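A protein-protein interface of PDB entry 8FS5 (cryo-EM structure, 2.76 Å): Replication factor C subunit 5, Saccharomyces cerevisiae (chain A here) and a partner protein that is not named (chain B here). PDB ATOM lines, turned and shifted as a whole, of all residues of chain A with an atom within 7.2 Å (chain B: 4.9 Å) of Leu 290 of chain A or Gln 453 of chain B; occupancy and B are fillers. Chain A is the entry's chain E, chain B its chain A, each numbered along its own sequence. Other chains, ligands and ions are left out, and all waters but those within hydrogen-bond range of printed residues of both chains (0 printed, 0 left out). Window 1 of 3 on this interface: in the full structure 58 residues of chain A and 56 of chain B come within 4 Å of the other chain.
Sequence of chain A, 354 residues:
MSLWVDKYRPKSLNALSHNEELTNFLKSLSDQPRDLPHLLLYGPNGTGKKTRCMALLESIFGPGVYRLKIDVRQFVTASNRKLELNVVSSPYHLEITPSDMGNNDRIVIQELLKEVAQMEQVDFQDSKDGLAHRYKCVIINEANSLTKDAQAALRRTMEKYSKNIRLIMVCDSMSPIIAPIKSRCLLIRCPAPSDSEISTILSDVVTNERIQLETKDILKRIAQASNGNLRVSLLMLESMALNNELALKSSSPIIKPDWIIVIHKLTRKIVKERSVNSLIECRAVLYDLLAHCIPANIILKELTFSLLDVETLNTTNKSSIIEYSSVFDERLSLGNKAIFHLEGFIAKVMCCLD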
ATOM      1  N   ARG A 283       0.660  16.194 -27.488  1.00  0.00           N
ATOM      2  CA  ARG A 283       1.428  15.952 -26.270  1.00  0.00           C
ATOM      3  C   ARG A 283       0.835  14.813 -25.452  1.00  0.00           C
ATOM      4  O   ARG A 283       1.582  14.015 -24.878  1.00  0.00           O
ATOM      5  CB  ARG A 283       1.514  17.220 -25.418  1.00  0.00           C
ATOM      6  CG  ARG A 283       2.392  17.043 -24.184  1.00  0.00           C
ATOM      7  CD  ARG A 283       2.875  18.361 -23.604  1.00  0.00           C
ATOM      8  NE  ARG A 283       1.805  19.114 -22.962  1.00  0.00           N
ATOM      9  CZ  ARG A 283       1.422  20.330 -23.326  1.00  0.00           C
ATOM     10  NH1 ARG A 283       2.005  20.966 -24.329  1.00  0.00           N
ATOM     11  NH2 ARG A 283       0.434  20.924 -22.663  1.00  0.00           N
ATOM     12  N   ALA A 284      -0.494  14.721 -25.382  1.00  0.00           N
ATOM     13  CA  ALA A 284      -1.133  13.606 -24.690  1.00  0.00           C
ATOM     14  C   ALA A 284      -0.813  12.279 -25.367  1.00  0.00           C
ATOM     15  O   ALA A 284      -0.532  11.279 -24.695  1.00  0.00           O
ATOM     16  CB  ALA A 284      -2.645  13.825 -24.624  1.00  0.00           C
ATOM     17  N   VAL A 285      -0.851  12.257 -26.702  1.00  0.00           N
ATOM     18  CA  VAL A 285      -0.507  11.039 -27.435  1.00  0.00           C
ATOM     19  C   VAL A 285       0.949  10.657 -27.186  1.00  0.00           C
ATOM     20  O   VAL A 285       1.275   9.479 -26.985  1.00  0.00           O
ATOM     21  CB  VAL A 285      -0.802  11.218 -28.937  1.00  0.00           C
ATOM     22  CG1 VAL A 285      -0.237  10.054 -29.738  1.00  0.00           C
ATOM     23  CG2 VAL A 285      -2.298  11.354 -29.169  1.00  0.00           C
ATOM     24  N   LEU A 286       1.848  11.647 -27.190  1.00  0.00           N
ATOM     25  CA  LEU A 286       3.260  11.382 -26.934  1.00  0.00           C
ATOM     26  C   LEU A 286       3.484  10.864 -25.520  1.00  0.00           C
ATOM     27  O   LEU A 286       4.304   9.965 -25.304  1.00  0.00           O
ATOM     28  CB  LEU A 286       4.085  12.646 -27.173  1.00  0.00           C
ATOM     29  CG  LEU A 286       4.293  13.085 -28.621  1.00  0.00           C
ATOM     30  CD1 LEU A 286       5.125  14.354 -28.665  1.00  0.00           C
ATOM     31  CD2 LEU A 286       4.950  11.978 -29.430  1.00  0.00           C
ATOM     32  N   TYR A 287       2.780  11.433 -24.538  1.00  0.00           N
ATOM     33  CA  TYR A 287       2.880  10.944 -23.167  1.00  0.00           C
ATOM     34  C   TYR A 287       2.375   9.513 -23.047  1.00  0.00           C
ATOM     35  O   TYR A 287       2.980   8.701 -22.337  1.00  0.00           O
ATOM     36  CB  TYR A 287       2.103  11.857 -22.220  1.00  0.00           C
ATOM     37  CG  TYR A 287       2.922  12.989 -21.643  1.00  0.00           C
ATOM     38  CD1 TYR A 287       4.182  12.757 -21.109  1.00  0.00           C
ATOM     39  CD2 TYR A 287       2.430  14.288 -21.624  1.00  0.00           C
ATOM     40  CE1 TYR A 287       4.933  13.788 -20.576  1.00  0.00           C
ATOM     41  CE2 TYR A 287       3.173  15.325 -21.094  1.00  0.00           C
ATOM     42  CZ  TYR A 287       4.423  15.069 -20.571  1.00  0.00           C
ATOM     43  OH  TYR A 287       5.167  16.098 -20.043  1.00  0.00           O
ATOM     44  N   ASP A 288       1.271   9.191 -23.724  1.00  0.00           N
ATOM     45  CA  ASP A 288       0.771   7.820 -23.715  1.00  0.00           C
ATOM     46  C   ASP A 288       1.774   6.864 -24.349  1.00  0.00           C
ATOM     47  O   ASP A 288       1.981   5.753 -23.849  1.00  0.00           O
ATOM     48  CB  ASP A 288      -0.575   7.747 -24.434  1.00  0.00           C
ATOM     49  CG  ASP A 288      -1.031   6.323 -24.674  1.00  0.00           C
ATOM     50  OD1 ASP A 288      -1.558   5.698 -23.729  1.00  0.00           O
ATOM     51  OD2 ASP A 288      -0.862   5.828 -25.807  1.00  0.00           O
ATOM     52  N   LEU A 289       2.404   7.278 -25.451  1.00  0.00           N
ATOM     53  CA  LEU A 289       3.421   6.442 -26.086  1.00  0.00           C
ATOM     54  C   LEU A 289       4.632   6.252 -25.179  1.00  0.00           C
ATOM     55  O   LEU A 289       5.179   5.146 -25.089  1.00  0.00           O
ATOM     56  CB  LEU A 289       3.846   7.053 -27.422  1.00  0.00           C
ATOM     57  CG  LEU A 289       2.860   6.923 -28.584  1.00  0.00           C
ATOM     58  CD1 LEU A 289       3.270   7.824 -29.737  1.00  0.00           C
ATOM     59  CD2 LEU A 289       2.758   5.476 -29.039  1.00  0.00           C
ATOM     60  N   LEU A 290       5.066   7.318 -24.503  1.00  0.00           N
ATOM     61  CA  LEU A 290       6.208   7.232 -23.602  1.00  0.00           C
ATOM     62  C   LEU A 290       5.902   6.414 -22.355  1.00  0.00           C
ATOM     63  O   LEU A 290       6.826   5.855 -21.755  1.00  0.00           O
ATOM     64  CB  LEU A 290       6.669   8.635 -23.201  1.00  0.00           C
ATOM     65  CG  LEU A 290       7.541   9.383 -24.210  1.00  0.00           C
ATOM     66  CD1 LEU A 290       7.769  10.817 -23.762  1.00  0.00           C
ATOM     67  CD2 LEU A 290       8.866   8.664 -24.413  1.00  0.00           C
ATOM     68  N   ALA A 291       4.633   6.337 -21.951  1.00  0.00           N
ATOM     69  CA  ALA A 291       4.255   5.521 -20.804  1.00  0.00           C
ATOM     70  C   ALA A 291       4.448   4.031 -21.052  1.00  0.00           C
ATOM     71  O   ALA A 291       4.471   3.255 -20.091  1.00  0.00           O
ATOM     72  CB  ALA A 291       2.799   5.794 -20.419  1.00  0.00           C
ATOM     73  N   HIS A 292       4.586   3.616 -22.312  1.00  0.00           N
ATOM     74  CA  HIS A 292       4.819   2.223 -22.661  1.00  0.00           C
ATOM     75  C   HIS A 292       6.298   1.906 -22.854  1.00  0.00           C
ATOM     76  O   HIS A 292       6.628   0.915 -23.516  1.00  0.00           O
ATOM     77  CB  HIS A 292       4.026   1.856 -23.917  1.00  0.00           C
ATOM     78  CG  HIS A 292       2.543   1.917 -23.727  1.00  0.00           C
ATOM     79  ND1 HIS A 292       1.857   1.020 -22.938  1.00  0.00           N
ATOM     80  CD2 HIS A 292       1.615   2.774 -24.214  1.00  0.00           C
ATOM     81  CE1 HIS A 292       0.570   1.318 -22.951  1.00  0.00           C
ATOM     82  NE2 HIS A 292       0.397   2.379 -23.718  1.00  0.00           N
ATOM     83  N   CYS A 293       7.185   2.738 -22.303  1.00  0.00           N
ATOM     84  CA  CYS A 293       8.629   2.486 -22.279  1.00  0.00           C
ATOM     85  C   CYS A 293       9.213   2.379 -23.686  1.00  0.00           C
ATOM     86  O   CYS A 293      10.201   1.681 -23.921  1.00  0.00           O
ATOM     87  CB  CYS A 293       8.954   1.236 -21.459  1.00  0.00           C
ATOM     88  SG  CYS A 293       8.482   1.351 -19.724  1.00  0.00           S
ATOM     89  N   ILE A 294       8.602   3.083 -24.631  1.00  0.00           N
ATOM     90  CA  ILE A 294       9.089   3.136 -26.006  1.00  0.00           C
ATOM     91  C   ILE A 294      10.108   4.269 -26.090  1.00  0.00           C
ATOM     92  O   ILE A 294       9.787   5.400 -25.693  1.00  0.00           O
ATOM     93  CB  ILE A 294       7.943   3.344 -27.003  1.00  0.00           C
ATOM     94  CG1 ILE A 294       7.286   2.006 -27.338  1.00  0.00           C
ATOM     95  CG2 ILE A 294       8.459   3.957 -28.287  1.00  0.00           C
ATOM     96  CD1 ILE A 294       5.810   2.111 -27.646  1.00  0.00           C
ATOM     97  N   PRO A 295      11.333   4.010 -26.553  1.00  0.00           N
ATOM     98  CA  PRO A 295      12.360   5.061 -26.569  1.00  0.00           C
ATOM     99  C   PRO A 295      11.953   6.244 -27.438  1.00  0.00           C
ATOM    100  O   PRO A 295      11.308   6.088 -28.478  1.00  0.00           O
ATOM    101  CB  PRO A 295      13.595   4.346 -27.134  1.00  0.00           C
ATOM    102  CG  PRO A 295      13.081   3.085 -27.756  1.00  0.00           C
ATOM    103  CD  PRO A 295      11.857   2.708 -26.992  1.00  0.00           C
ATOM    104  N   ALA A 296      12.345   7.439 -26.995  1.00  0.00           N
ATOM    105  CA  ALA A 296      11.953   8.679 -27.651  1.00  0.00           C
ATOM    106  C   ALA A 296      12.605   8.876 -29.012  1.00  0.00           C
ATOM    107  O   ALA A 296      11.992   9.502 -29.884  1.00  0.00           O
ATOM    108  CB  ALA A 296      12.282   9.871 -26.755  1.00  0.00           C
ATOM    109  N   ASN A 297      13.826   8.376 -29.210  1.00  0.00           N
ATOM    110  CA  ASN A 297      14.470   8.468 -30.515  1.00  0.00           C
ATOM    111  C   ASN A 297      13.696   7.724 -31.592  1.00  0.00           C
ATOM    112  O   ASN A 297      13.534   8.251 -32.699  1.00  0.00           O
ATOM    113  CB  ASN A 297      15.900   7.929 -30.436  1.00  0.00           C
ATOM    114  CG  ASN A 297      16.023   6.740 -29.504  1.00  0.00           C
ATOM    115  OD1 ASN A 297      15.831   6.863 -28.294  1.00  0.00           O
ATOM    116  ND2 ASN A 297      16.346   5.580 -30.063  1.00  0.00           N
ATOM    117  N   ILE A 299      10.420   7.105 -31.435  1.00  0.00           N
ATOM    118  CA  ILE A 299       9.199   7.879 -31.643  1.00  0.00           C
ATOM    119  C   ILE A 299       9.425   8.976 -32.671  1.00  0.00           C
ATOM    120  O   ILE A 299       8.654   9.101 -33.629  1.00  0.00           O
ATOM    121  CB  ILE A 299       8.697   8.474 -30.317  1.00  0.00           C
ATOM    122  CG1 ILE A 299       8.422   7.368 -29.299  1.00  0.00           C
ATOM    123  CG2 ILE A 299       7.453   9.324 -30.555  1.00  0.00           C
ATOM    124  CD1 ILE A 299       7.564   7.801 -28.128  1.00  0.00           C
ATOM    125  N   ALA A 338      12.617  14.109 -22.510  1.00  0.00           N
ATOM    126  CA  ALA A 338      12.349  13.952 -23.934  1.00  0.00           C
ATOM    127  C   ALA A 338      11.085  14.663 -24.395  1.00  0.00           C
ATOM    128  O   ALA A 338      10.929  14.908 -25.599  1.00  0.00           O
ATOM    129  CB  ALA A 338      12.241  12.466 -24.280  1.00  0.00           C
ATOM    130  N   ILE A 339      10.182  14.996 -23.469  1.00  0.00           N
ATOM    131  CA  ILE A 339       8.911  15.600 -23.857  1.00  0.00           C
ATOM    132  C   ILE A 339       9.124  16.974 -24.476  1.00  0.00           C
ATOM    133  O   ILE A 339       8.415  17.353 -25.416  1.00  0.00           O
ATOM    134  CB  ILE A 339       7.946  15.648 -22.652  1.00  0.00           C
ATOM    135  CG1 ILE A 339       6.557  16.120 -23.093  1.00  0.00           C
ATOM    136  CG2 ILE A 339       8.501  16.510 -21.521  1.00  0.00           C
ATOM    137  CD1 ILE A 339       5.954  15.292 -24.207  1.00  0.00           C
ATOM    138  N   LEU A 342      10.323  16.299 -28.110  1.00  0.00           N
ATOM    139  CA  LEU A 342       9.249  15.648 -28.849  1.00  0.00           C
ATOM    140  C   LEU A 342       8.072  16.576 -29.112  1.00  0.00           C
ATOM    141  O   LEU A 342       7.374  16.396 -30.117  1.00  0.00           O
ATOM    142  CB  LEU A 342       8.769  14.404 -28.098  1.00  0.00           C
ATOM    143  CG  LEU A 342       9.707  13.196 -28.116  1.00  0.00           C
ATOM    144  CD1 LEU A 342       9.199  12.107 -27.184  1.00  0.00           C
ATOM    145  CD2 LEU A 342       9.870  12.663 -29.531  1.00  0.00           C
ATOM    146  N   VAL B 449       3.169   9.354 -15.863  1.00  0.00           N
ATOM    147  CA  VAL B 449       3.902   8.633 -16.898  1.00  0.00           C
ATOM    148  C   VAL B 449       5.023   7.807 -16.288  1.00  0.00           C
ATOM    149  O   VAL B 449       5.256   6.666 -16.699  1.00  0.00           O
ATOM    150  CB  VAL B 449       4.435   9.620 -17.955  1.00  0.00           C
ATOM    151  CG1 VAL B 449       5.120   8.871 -19.087  1.00  0.00           C
ATOM    152  CG2 VAL B 449       3.303  10.482 -18.487  1.00  0.00           C
ATOM    153  N   ARG B 450       5.726   8.354 -15.298  1.00  0.00           N
ATOM    154  CA  ARG B 450       6.818   7.634 -14.656  1.00  0.00           C
ATOM    155  C   ARG B 450       6.346   6.430 -13.850  1.00  0.00           C
ATOM    156  O   ARG B 450       7.050   5.415 -13.820  1.00  0.00           O
ATOM    157  CB  ARG B 450       7.615   8.582 -13.756  1.00  0.00           C
ATOM    158  CG  ARG B 450       8.534   9.517 -14.528  1.00  0.00           C
ATOM    159  CD  ARG B 450       9.916   9.599 -13.902  1.00  0.00           C
ATOM    160  NE  ARG B 450      10.528   8.283 -13.769  1.00  0.00           N
ATOM    161  CZ  ARG B 450      11.675   7.930 -14.330  1.00  0.00           C
ATOM    162  NH1 ARG B 450      12.364   8.773 -15.083  1.00  0.00           N
ATOM    163  NH2 ARG B 450      12.142   6.700 -14.135  1.00  0.00           N
ATOM    164  N   LYS B 451       5.183   6.509 -13.203  1.00  0.00           N
ATOM    165  CA  LYS B 451       4.599   5.347 -12.542  1.00  0.00           C
ATOM    166  C   LYS B 451       4.035   4.316 -13.509  1.00  0.00           C
ATOM    167  O   LYS B 451       4.178   3.112 -13.261  1.00  0.00           O
ATOM    168  CB  LYS B 451       3.489   5.768 -11.566  1.00  0.00           C
ATOM    169  CG  LYS B 451       3.905   6.839 -10.560  1.00  0.00           C
ATOM    170  CD  LYS B 451       2.870   7.055  -9.453  1.00  0.00           C
ATOM    171  CE  LYS B 451       2.355   5.770  -8.794  1.00  0.00           C
ATOM    172  NZ  LYS B 451       3.352   4.663  -8.660  1.00  0.00           N
ATOM    173  N   LEU B 452       3.402   4.747 -14.603  1.00  0.00           N
ATOM    174  CA  LEU B 452       3.008   3.811 -15.646  1.00  0.00           C
ATOM    175  C   LEU B 452       4.207   3.124 -16.281  1.00  0.00           C
ATOM    176  O   LEU B 452       4.102   1.959 -16.674  1.00  0.00           O
ATOM    177  CB  LEU B 452       2.187   4.526 -16.721  1.00  0.00           C
ATOM    178  CG  LEU B 452       0.754   4.904 -16.342  1.00  0.00           C
ATOM    179  CD1 LEU B 452       0.318   6.163 -17.075  1.00  0.00           C
ATOM    180  CD2 LEU B 452      -0.202   3.755 -16.628  1.00  0.00           C
ATOM    181  N   GLN B 453       5.345   3.816 -16.373  1.00  0.00           N
ATOM    182  CA  GLN B 453       6.566   3.199 -16.878  1.00  0.00           C
ATOM    183  C   GLN B 453       7.043   2.091 -15.944  1.00  0.00           C
ATOM    184  O   GLN B 453       7.474   1.024 -16.395  1.00  0.00           O
ATOM    185  CB  GLN B 453       7.649   4.266 -17.056  1.00  0.00           C
ATOM    186  CG  GLN B 453       7.888   4.669 -18.501  1.00  0.00           C
ATOM    187  CD  GLN B 453       8.794   5.877 -18.628  1.00  0.00           C
ATOM    188  OE1 GLN B 453       9.624   6.140 -17.758  1.00  0.00           O
ATOM    189  NE2 GLN B 453       8.638   6.621 -19.716  1.00  0.00           N
ATOM    190  N   ASN B 454       6.973   2.326 -14.631  1.00  0.00           N
ATOM    191  CA  ASN B 454       7.333   1.290 -13.669  1.00  0.00           C
ATOM    192  C   ASN B 454       6.372   0.109 -13.711  1.00  0.00           C
ATOM    193  O   ASN B 454       6.813  -1.042 -13.598  1.00  0.00           O
ATOM    194  CB  ASN B 454       7.382   1.876 -12.258  1.00  0.00           C
ATOM    195  CG  ASN B 454       8.341   3.044 -12.148  1.00  0.00           C
ATOM    196  OD1 ASN B 454       9.183   3.255 -13.020  1.00  0.00           O
ATOM    197  ND2 ASN B 454       8.218   3.811 -11.071  1.00  0.00           N
ATOM    198  N   SER B 455       5.073   0.365 -13.869  1.00  0.00           N
ATOM    199  CA  SER B 455       4.121  -0.722 -14.075  1.00  0.00           C
ATOM    200  C   SER B 455       4.415  -1.512 -15.346  1.00  0.00           C
ATOM    201  O   SER B 455       4.318  -2.748 -15.333  1.00  0.00           O
ATOM    202  CB  SER B 455       2.693  -0.173 -14.126  1.00  0.00           C
ATOM    203  OG  SER B 455       2.461   0.532 -15.332  1.00  0.00           O
ATOM    204  N   PHE B 456       4.773  -0.823 -16.432  1.00  0.00           N
ATOM    205  CA  PHE B 456       5.188  -1.491 -17.660  1.00  0.00           C
ATOM    206  C   PHE B 456       6.417  -2.356 -17.417  1.00  0.00           C
ATOM    207  O   PHE B 456       6.512  -3.474 -17.930  1.00  0.00           O
ATOM    208  CB  PHE B 456       5.461  -0.449 -18.751  1.00  0.00           C
ATOM    209  CG  PHE B 456       5.603  -1.029 -20.136  1.00  0.00           C
ATOM    210  CD1 PHE B 456       6.780  -1.644 -20.535  1.00  0.00           C
ATOM    211  CD2 PHE B 456       4.562  -0.943 -21.044  1.00  0.00           C
ATOM    212  CE1 PHE B 456       6.910  -2.172 -21.805  1.00  0.00           C
ATOM    213  CE2 PHE B 456       4.688  -1.467 -22.317  1.00  0.00           C
ATOM    214  CZ  PHE B 456       5.862  -2.083 -22.697  1.00  0.00           C
ATOM    215  N   LYS B 457       7.381  -1.843 -16.650  1.00  0.00           N
ATOM    216  CA  LYS B 457       8.583  -2.601 -16.321  1.00  0.00           C
ATOM    217  C   LYS B 457       8.244  -3.871 -15.548  1.00  0.00           C
ATOM    218  O   LYS B 457       8.776  -4.951 -15.829  1.00  0.00           O
ATOM    219  CB  LYS B 457       9.547  -1.729 -15.510  1.00  0.00           C
ATOM    220  CG  LYS B 457      10.782  -1.270 -16.268  1.00  0.00           C
ATOM    221  CD  LYS B 457      10.480  -0.068 -17.140  1.00  0.00           C
ATOM    222  CE  LYS B 457      11.754   0.532 -17.710  1.00  0.00           C
ATOM    223  NZ  LYS B 457      12.476   1.353 -16.699  1.00  0.00           N
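The backbone carbonyl oxygen (O) of Gln 453 of chain B lies within hydrogen-bond range of the side-chain sulfur (SG) of Cys 293 of chain A, 3.5 Å away.
The side-chain amide nitrogen of Gln 453 of chain B lies within hydrogen-bond range of the backbone carbonyl oxygen of Leu 290 of chain A (2.8 Å).
The backbone carbonyl oxygen (O) of Leu 452 of chain B lies within hydrogen-bond range of the side-chain hydroxyl (OG) of Ser 455 of chain B, at 2.6 Å.
Among the printed residues, merely in contact across the chains: Tyr 287 of chain A with Val 449 of chain B (3.6 Å), Ala 291 of chain A with Val 449 of chain B (3.9 Å), Ala 291 of chain A with Leu 452 of chain B (3.7 Å), Ala 291 of chain A with Gln 453 of chain B (3.8 Å), His 292 of chain A with Phe 456 of chain B (3.2 Å), Cys 293 of chain A with Phe 456 of chain B (3.5 Å) and Cys 293 of chain A with Lys 457 of chain B (3.6 Å).
Of chain B, only Gln 453 comes within 4 Å of Leu 290 of chain A.
Of chain A, only Leu 290 (2.8 Å), Ala 291 (3.8 Å) and Cys 293 (3.5 Å) come within 4 Å of Gln 453 of chain B.
Of the printed residues of chain A, Lys 457 of chain B touches Cys 293.
Of the printed residues of chain A, Val 449 of chain B touches Tyr 287 and Ala 291.
Asp 288 of chain A touches none of the printed residues of chain B.
The nearest residue of chain B that does not touch Leu 290 of chain A is Val 449 of chain B (4.2 Å).
The nearest residue of chain A that does not touch Gln 453 of chain B is His 292 of chain A (5.2 Å).
The nearest printed residue of chain B that does not touch His 292 of chain A is Gln 453 of chain B (5.2 Å).
Printed residues of chain B that touch a printed residue of chain A: Val 449, Leu 452, Gln 453, Phe 456 and Lys 457.
Hydrophobic or aromatic side chains of chain B that line the printed part of chain A: Val 449, Leu 452 and Phe 456.
Of the 19 printed residues of chain A, 5 touch a printed residue of chain B.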
